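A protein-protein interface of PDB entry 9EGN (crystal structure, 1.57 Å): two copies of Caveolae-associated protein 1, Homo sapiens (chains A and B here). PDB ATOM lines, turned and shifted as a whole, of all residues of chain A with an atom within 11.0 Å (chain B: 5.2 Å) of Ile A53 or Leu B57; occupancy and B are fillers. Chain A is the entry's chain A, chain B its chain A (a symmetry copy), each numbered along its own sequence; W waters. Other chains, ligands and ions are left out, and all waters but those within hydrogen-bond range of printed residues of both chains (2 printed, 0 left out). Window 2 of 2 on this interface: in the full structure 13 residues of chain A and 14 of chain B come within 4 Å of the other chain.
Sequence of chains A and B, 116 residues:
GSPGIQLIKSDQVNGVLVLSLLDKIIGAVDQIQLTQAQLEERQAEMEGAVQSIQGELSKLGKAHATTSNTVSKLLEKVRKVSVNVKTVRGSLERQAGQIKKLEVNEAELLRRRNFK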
ATOM      1  N   GLU A  45     -33.121  18.404 -16.957  1.00  0.00           N
ATOM      2  CA  GLU A  45     -32.579  17.375 -17.842  1.00  0.00           C
ATOM      3  C   GLU A  45     -31.902  18.006 -19.053  1.00  0.00           C
ATOM      4  O   GLU A  45     -30.779  17.644 -19.417  1.00  0.00           O
ATOM      5  CB  GLU A  45     -33.734  16.500 -18.321  1.00  0.00           C
ATOM      6  CG  GLU A  45     -34.428  15.718 -17.191  1.00  0.00           C
ATOM      7  CD  GLU A  45     -35.700  14.999 -17.643  1.00  0.00           C
ATOM      8  OE1 GLU A  45     -36.321  15.429 -18.647  1.00  0.00           O
ATOM      9  OE2 GLU A  45     -36.090  14.019 -16.972  1.00  0.00           O
ATOM     10  N   MET A  46     -32.564  19.002 -19.634  1.00  0.00           N
ATOM     11  CA  MET A  46     -32.032  19.688 -20.832  1.00  0.00           C
ATOM     12  C   MET A  46     -30.832  20.561 -20.463  1.00  0.00           C
ATOM     13  O   MET A  46     -30.029  20.715 -21.321  1.00  0.00           O
ATOM     14  CB  MET A  46     -33.093  20.575 -21.476  1.00  0.00           C
ATOM     15  CG  MET A  46     -32.826  20.871 -22.925  1.00  0.00           C
ATOM     16  SD  MET A  46     -33.455  22.502 -23.343  1.00  0.00           S
ATOM     17  CE  MET A  46     -35.147  21.949 -23.585  1.00  0.00           C
ATOM     18  N   GLU A  47     -30.779  21.186 -19.293  1.00  0.00           N
ATOM     19  CA  GLU A  47     -29.611  21.955 -18.866  1.00  0.00           C
ATOM     20  C   GLU A  47     -28.389  21.071 -18.674  1.00  0.00           C
ATOM     21  O   GLU A  47     -27.268  21.487 -18.989  1.00  0.00           O
ATOM     22  CB  GLU A  47     -29.953  22.738 -17.588  1.00  0.00           C
ATOM     23  CG  GLU A  47     -30.727  24.029 -17.885  1.00  0.00           C
ATOM     24  CD  GLU A  47     -31.494  24.607 -16.688  1.00  0.00           C
ATOM     25  OE1 GLU A  47     -31.530  23.959 -15.612  1.00  0.00           O
ATOM     26  OE2 GLU A  47     -32.131  25.674 -16.856  1.00  0.00           O
ATOM     27  N   GLY A  48     -28.573  19.851 -18.175  1.00  0.00           N
ATOM     28  CA  GLY A  48     -27.471  18.902 -18.143  1.00  0.00           C
ATOM     29  C   GLY A  48     -26.988  18.505 -19.528  1.00  0.00           C
ATOM     30  O   GLY A  48     -25.783  18.393 -19.769  1.00  0.00           O
ATOM     31  N   ALA A  49     -27.922  18.270 -20.449  1.00  0.00           N
ATOM     32  CA  ALA A  49     -27.551  17.921 -21.819  1.00  0.00           C
ATOM     33  C   ALA A  49     -26.805  19.048 -22.521  1.00  0.00           C
ATOM     34  O   ALA A  49     -25.803  18.803 -23.208  1.00  0.00           O
ATOM     35  CB  ALA A  49     -28.793  17.554 -22.622  1.00  0.00           C
ATOM     36  N   VAL A  50     -27.260  20.289 -22.353  1.00  0.00           N
ATOM     37  CA  VAL A  50     -26.564  21.424 -22.952  1.00  0.00           C
ATOM     38  C   VAL A  50     -25.184  21.604 -22.339  1.00  0.00           C
ATOM     39  O   VAL A  50     -24.216  21.889 -23.053  1.00  0.00           O
ATOM     40  CB  VAL A  50     -27.416  22.706 -22.837  1.00  0.00           C
ATOM     41  CG1 VAL A  50     -26.604  23.947 -23.215  1.00  0.00           C
ATOM     42  CG2 VAL A  50     -28.612  22.612 -23.752  1.00  0.00           C
ATOM     43  N   GLN A  51     -25.066  21.472 -21.016  1.00  0.00           N
ATOM     44  CA  GLN A  51     -23.748  21.558 -20.385  1.00  0.00           C
ATOM     45  C   GLN A  51     -22.794  20.478 -20.884  1.00  0.00           C
ATOM     46  O   GLN A  51     -21.589  20.724 -21.024  1.00  0.00           O
ATOM     47  CB  GLN A  51     -23.892  21.482 -18.866  1.00  0.00           C
ATOM     48  CG  GLN A  51     -24.419  22.774 -18.312  1.00  0.00           C
ATOM     49  CD  GLN A  51     -24.862  22.679 -16.873  1.00  0.00           C
ATOM     50  OE1 GLN A  51     -24.710  21.643 -16.221  1.00  0.00           O
ATOM     51  NE2 GLN A  51     -25.438  23.762 -16.373  1.00  0.00           N
ATOM     52  N   SER A  52     -23.303  19.279 -21.147  1.00  0.00           N
ATOM     53  CA  SER A  52     -22.460  18.234 -21.717  1.00  0.00           C
ATOM     54  C   SER A  52     -21.983  18.576 -23.127  1.00  0.00           C
ATOM     55  O   SER A  52     -20.805  18.382 -23.445  1.00  0.00           O
ATOM     56  CB  SER A  52     -23.224  16.915 -21.749  1.00  0.00           C
ATOM     57  OG  SER A  52     -23.075  16.226 -20.522  1.00  0.00           O
ATOM     58  N   ILE A  53     -22.847  19.160 -23.949  1.00  0.00           N
ATOM     59  CA  ILE A  53     -22.434  19.604 -25.284  1.00  0.00           C
ATOM     60  C   ILE A  53     -21.412  20.731 -25.191  1.00  0.00           C
ATOM     61  O   ILE A  53     -20.402  20.744 -25.910  1.00  0.00           O
ATOM     62  CB  ILE A  53     -23.674  20.041 -26.091  1.00  0.00           C
ATOM     63  CG1 ILE A  53     -24.566  18.856 -26.403  1.00  0.00           C
ATOM     64  CG2 ILE A  53     -23.283  20.740 -27.388  1.00  0.00           C
ATOM     65  CD1 ILE A  53     -26.007  19.234 -26.732  1.00  0.00           C
ATOM     66  N   GLN A  54     -21.658  21.700 -24.320  1.00  0.00           N
ATOM     67  CA  GLN A  54     -20.727  22.802 -24.128  1.00  0.00           C
ATOM     68  C   GLN A  54     -19.355  22.312 -23.685  1.00  0.00           C
ATOM     69  O   GLN A  54     -18.329  22.812 -24.155  1.00  0.00           O
ATOM     70  CB  GLN A  54     -21.325  23.747 -23.087  1.00  0.00           C
ATOM     71  CG  GLN A  54     -22.445  24.596 -23.619  1.00  0.00           C
ATOM     72  CD  GLN A  54     -23.043  25.488 -22.538  1.00  0.00           C
ATOM     73  OE1 GLN A  54     -22.999  25.144 -21.353  1.00  0.00           O
ATOM     74  NE2 GLN A  54     -23.605  26.605 -22.937  1.00  0.00           N
ATOM     75  N   GLY A  55     -19.316  21.310 -22.813  1.00  0.00           N
ATOM     76  CA  GLY A  55     -18.040  20.727 -22.426  1.00  0.00           C
ATOM     77  C   GLY A  55     -17.334  20.027 -23.568  1.00  0.00           C
ATOM     78  O   GLY A  55     -16.113  20.138 -23.719  1.00  0.00           O
ATOM     79  N   GLU A  56     -18.093  19.308 -24.391  1.00  0.00           N
ATOM     80  CA  GLU A  56     -17.528  18.674 -25.578  1.00  0.00           C
ATOM     81  C   GLU A  56     -16.929  19.669 -26.567  1.00  0.00           C
ATOM     82  O   GLU A  56     -15.831  19.443 -27.099  1.00  0.00           O
ATOM     83  CB  GLU A  56     -18.634  17.847 -26.232  1.00  0.00           C
ATOM     84  CG  GLU A  56     -18.260  17.274 -27.552  1.00  0.00           C
ATOM     85  CD  GLU A  56     -17.286  16.134 -27.425  1.00  0.00           C
ATOM     86  OE1 GLU A  56     -16.968  15.763 -26.284  1.00  0.00           O
ATOM     87  OE2 GLU A  56     -16.837  15.609 -28.469  1.00  0.00           O
ATOM     88  N   LEU A  57     -17.580  20.801 -26.779  1.00  0.00           N
ATOM     89  CA  LEU A  57     -17.078  21.810 -27.700  1.00  0.00           C
ATOM     90  C   LEU A  57     -15.982  22.685 -27.107  1.00  0.00           C
ATOM     91  O   LEU A  57     -15.448  23.527 -27.833  1.00  0.00           O
ATOM     92  CB  LEU A  57     -18.233  22.670 -28.195  1.00  0.00           C
ATOM     93  CG  LEU A  57     -19.287  21.919 -29.003  1.00  0.00           C
ATOM     94  CD1 LEU A  57     -20.449  22.821 -29.376  1.00  0.00           C
ATOM     95  CD2 LEU A  57     -18.651  21.336 -30.251  1.00  0.00           C
ATOM     96  N   SER A  58     -15.757  22.614 -25.793  1.00  0.00           N
ATOM     97  CA  SER A  58     -14.797  23.453 -25.080  1.00  0.00           C
ATOM     98  C   SER A  58     -13.519  22.730 -24.659  1.00  0.00           C
ATOM     99  O   SER A  58     -12.558  23.397 -24.257  1.00  0.00           O
ATOM    100  CB  SER A  58     -15.441  24.076 -23.838  1.00  0.00           C
ATOM    101  OG  SER A  58     -16.577  24.836 -24.194  1.00  0.00           O
ATOM    102  N   LYS A  59     -13.489  21.405 -24.693  1.00  0.00           N
ATOM    103  CA  LYS A  59     -12.343  20.654 -24.201  1.00  0.00           C
ATOM    104  C   LYS A  59     -11.103  20.914 -25.059  1.00  0.00           C
ATOM    105  O   LYS A  59     -11.186  21.362 -26.204  1.00  0.00           O
ATOM    106  CB  LYS A  59     -12.707  19.184 -24.115  1.00  0.00           C
ATOM    107  CG  LYS A  59     -12.859  18.503 -25.447  1.00  0.00           C
ATOM    108  CD  LYS A  59     -13.441  17.123 -25.230  1.00  0.00           C
ATOM    109  CE  LYS A  59     -13.490  16.315 -26.507  1.00  0.00           C
ATOM    110  NZ  LYS A  59     -14.163  15.008 -26.271  1.00  0.00           N
ATOM    111  N   LEU A  60      -9.936  20.644 -24.484  1.00  0.00           N
ATOM    112  CA  LEU A  60      -8.702  20.869 -25.231  1.00  0.00           C
ATOM    113  C   LEU A  60      -8.451  19.766 -26.258  1.00  0.00           C
ATOM    114  O   LEU A  60      -8.733  18.593 -26.014  1.00  0.00           O
ATOM    115  CB  LEU A  60      -7.506  20.963 -24.283  1.00  0.00           C
ATOM    116  CG  LEU A  60      -7.704  22.014 -23.177  1.00  0.00           C
ATOM    117  CD1 LEU A  60      -6.422  22.197 -22.325  1.00  0.00           C
ATOM    118  CD2 LEU A  60      -8.359  23.335 -23.619  1.00  0.00           C
ATOM    119  N   VAL B  50     -31.888  20.328 -29.395  1.00  0.00           N
ATOM    120  CA  VAL B  50     -30.817  19.648 -28.672  1.00  0.00           C
ATOM    121  C   VAL B  50     -30.619  18.233 -29.195  1.00  0.00           C
ATOM    122  O   VAL B  50     -29.480  17.776 -29.342  1.00  0.00           O
ATOM    123  CB  VAL B  50     -31.087  19.668 -27.153  1.00  0.00           C
ATOM    124  CG1 VAL B  50     -30.125  18.741 -26.407  1.00  0.00           C
ATOM    125  CG2 VAL B  50     -30.922  21.070 -26.620  1.00  0.00           C
ATOM    126  N   ILE B  53     -28.571  18.404 -32.326  1.00  0.00           N
ATOM    127  CA  ILE B  53     -27.150  18.614 -32.034  1.00  0.00           C
ATOM    128  C   ILE B  53     -26.505  17.333 -31.517  1.00  0.00           C
ATOM    129  O   ILE B  53     -25.394  16.964 -31.924  1.00  0.00           O
ATOM    130  CB  ILE B  53     -26.995  19.765 -31.018  1.00  0.00           C
ATOM    131  CG1 ILE B  53     -27.402  21.090 -31.632  1.00  0.00           C
ATOM    132  CG2 ILE B  53     -25.568  19.862 -30.493  1.00  0.00           C
ATOM    133  CD1 ILE B  53     -27.762  22.162 -30.607  1.00  0.00           C
ATOM    134  N   GLN B  54     -27.177  16.642 -30.607  1.00  0.00           N
ATOM    135  CA  GLN B  54     -26.666  15.387 -30.077  1.00  0.00           C
ATOM    136  C   GLN B  54     -26.458  14.353 -31.175  1.00  0.00           C
ATOM    137  O   GLN B  54     -25.456  13.633 -31.177  1.00  0.00           O
ATOM    138  CB  GLN B  54     -27.662  14.875 -29.037  1.00  0.00           C
ATOM    139  CG  GLN B  54     -27.601  15.617 -27.732  1.00  0.00           C
ATOM    140  CD  GLN B  54     -28.639  15.108 -26.741  1.00  0.00           C
ATOM    141  OE1 GLN B  54     -29.688  14.598 -27.145  1.00  0.00           O
ATOM    142  NE2 GLN B  54     -28.363  15.256 -25.465  1.00  0.00           N
ATOM    143  N   GLY B  55     -27.372  14.292 -32.140  1.00  0.00           N
ATOM    144  CA  GLY B  55     -27.182  13.398 -33.272  1.00  0.00           C
ATOM    145  C   GLY B  55     -26.000  13.779 -34.139  1.00  0.00           C
ATOM    146  O   GLY B  55     -25.247  12.913 -34.596  1.00  0.00           O
ATOM    147  N   GLU B  56     -25.817  15.077 -34.367  1.00  0.00           N
ATOM    148  CA  GLU B  56     -24.656  15.557 -35.108  1.00  0.00           C
ATOM    149  C   GLU B  56     -23.328  15.213 -34.438  1.00  0.00           C
ATOM    150  O   GLU B  56     -22.378  14.782 -35.110  1.00  0.00           O
ATOM    151  CB  GLU B  56     -24.808  17.067 -35.281  1.00  0.00           C
ATOM    152  CG  GLU B  56     -23.616  17.731 -35.871  1.00  0.00           C
ATOM    153  CD  GLU B  56     -23.463  17.434 -37.339  1.00  0.00           C
ATOM    154  OE1 GLU B  56     -24.344  16.758 -37.891  1.00  0.00           O
ATOM    155  OE2 GLU B  56     -22.458  17.877 -37.939  1.00  0.00           O
ATOM    156  N   LEU B  57     -23.251  15.321 -33.122  1.00  0.00           N
ATOM    157  CA  LEU B  57     -22.027  15.007 -32.400  1.00  0.00           C
ATOM    158  C   LEU B  57     -21.818  13.515 -32.175  1.00  0.00           C
ATOM    159  O   LEU B  57     -20.776  13.146 -31.627  1.00  0.00           O
ATOM    160  CB  LEU B  57     -22.013  15.751 -31.071  1.00  0.00           C
ATOM    161  CG  LEU B  57     -21.994  17.272 -31.192  1.00  0.00           C
ATOM    162  CD1 LEU B  57     -22.079  17.939 -29.830  1.00  0.00           C
ATOM    163  CD2 LEU B  57     -20.735  17.710 -31.915  1.00  0.00           C
ATOM    164  N   SER B  58     -22.834  12.688 -32.431  1.00  0.00           N
ATOM    165  CA  SER B  58     -22.802  11.249 -32.184  1.00  0.00           C
ATOM    166  C   SER B  58     -22.666  10.395 -33.442  1.00  0.00           C
ATOM    167  O   SER B  58     -22.402   9.193 -33.326  1.00  0.00           O
ATOM    168  CB  SER B  58     -24.051  10.803 -31.419  1.00  0.00           C
ATOM    169  OG  SER B  58     -24.164  11.503 -30.198  1.00  0.00           O
ATOM    170  N   LYS B  59     -22.878  10.956 -34.625  1.00  0.00           N
ATOM    171  CA  LYS B  59     -22.874  10.174 -35.853  1.00  0.00           C
ATOM    172  C   LYS B  59     -21.483   9.603 -36.139  1.00  0.00           C
ATOM    173  O   LYS B  59     -20.468  10.076 -35.627  1.00  0.00           O
ATOM    174  CB  LYS B  59     -23.411  11.023 -36.989  1.00  0.00           C
ATOM    175  CG  LYS B  59     -22.490  12.127 -37.430  1.00  0.00           C
ATOM    176  CD  LYS B  59     -23.229  13.029 -38.395  1.00  0.00           C
ATOM    177  CE  LYS B  59     -22.328  14.081 -38.998  1.00  0.00           C
ATOM    178  NZ  LYS B  59     -23.113  15.009 -39.858  1.00  0.00           N
HETATM  179  O   HOH W   1     -18.569  14.652 -30.661  1.00  0.00           O
HETATM  180  O   HOH W   2     -25.764  16.103 -24.373  1.00  0.00           O
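O of Gln B54 is in hydrogen-bond range of OG of Ser B58, 2.7 Å away.
Ala A49 touches Gln B54 (CB to NE2, 3.7 Å).
Val A50 touches Val B50 (CG2 to CG2, 3.99 Å).
Ile A53 touches Ile B53.
CG2 of Ile A53 touches CD1 of Leu B57, at 3.9 Å.
Of the printed residues of chain B, Ala A49 touches Gln B54.
Of the printed residues of chain B, Val A50 touches Val B50 (3.99 Å).
Ile A53 touches two residues of chain B.
Of the printed residues of chain A, Val B50 touches Val A50.
Gln B54 touches just one residue of chain A: Ala A49 (3.7 Å).
No residue of chain A comes within 4 Å of Glu B56.
No residue of chain A comes within 4 Å of Ser B58.
No residue of chain A comes within 4 Å of Lys B59.
The nearest residue of chain B that does not touch Ile A53 is Gln B54 (4.1 Å).
Of the 8 printed residues of chain B, 4 touch a printed residue of chain A.
Hydrophobic or aromatic side chains of chain B that line the printed part of chain A: Val B50, Ile B53 and Leu B57.
Among the printed residues, no Asp or Glu carboxylate lies within 4 Å of a Lys or Arg side-chain nitrogen of the other chain.
Val A50 touches its own counterpart, Val B50.
Ile A53 touches its own counterpart, Ile B53.
Ile A53 touches Leu B57, but with the chains exchanged Leu A57 does not touch Ile B53 (6.0 Å).
Of the 4 pairs that touch across the chains among the printed residues, 2 have their exchanged pair printed and touching as well.
Water W1 lies within hydrogen-bond range of O of Leu B57 (2.8 Å) and OE2 of Glu A56 (3.0 Å).
Water W2 lies within hydrogen-bond range of the backbone carbonyl oxygen (O) of Ala A49 (2.9 Å) and the side-chain amide nitrogen (NE2) of Gln B54 (2.9 Å).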
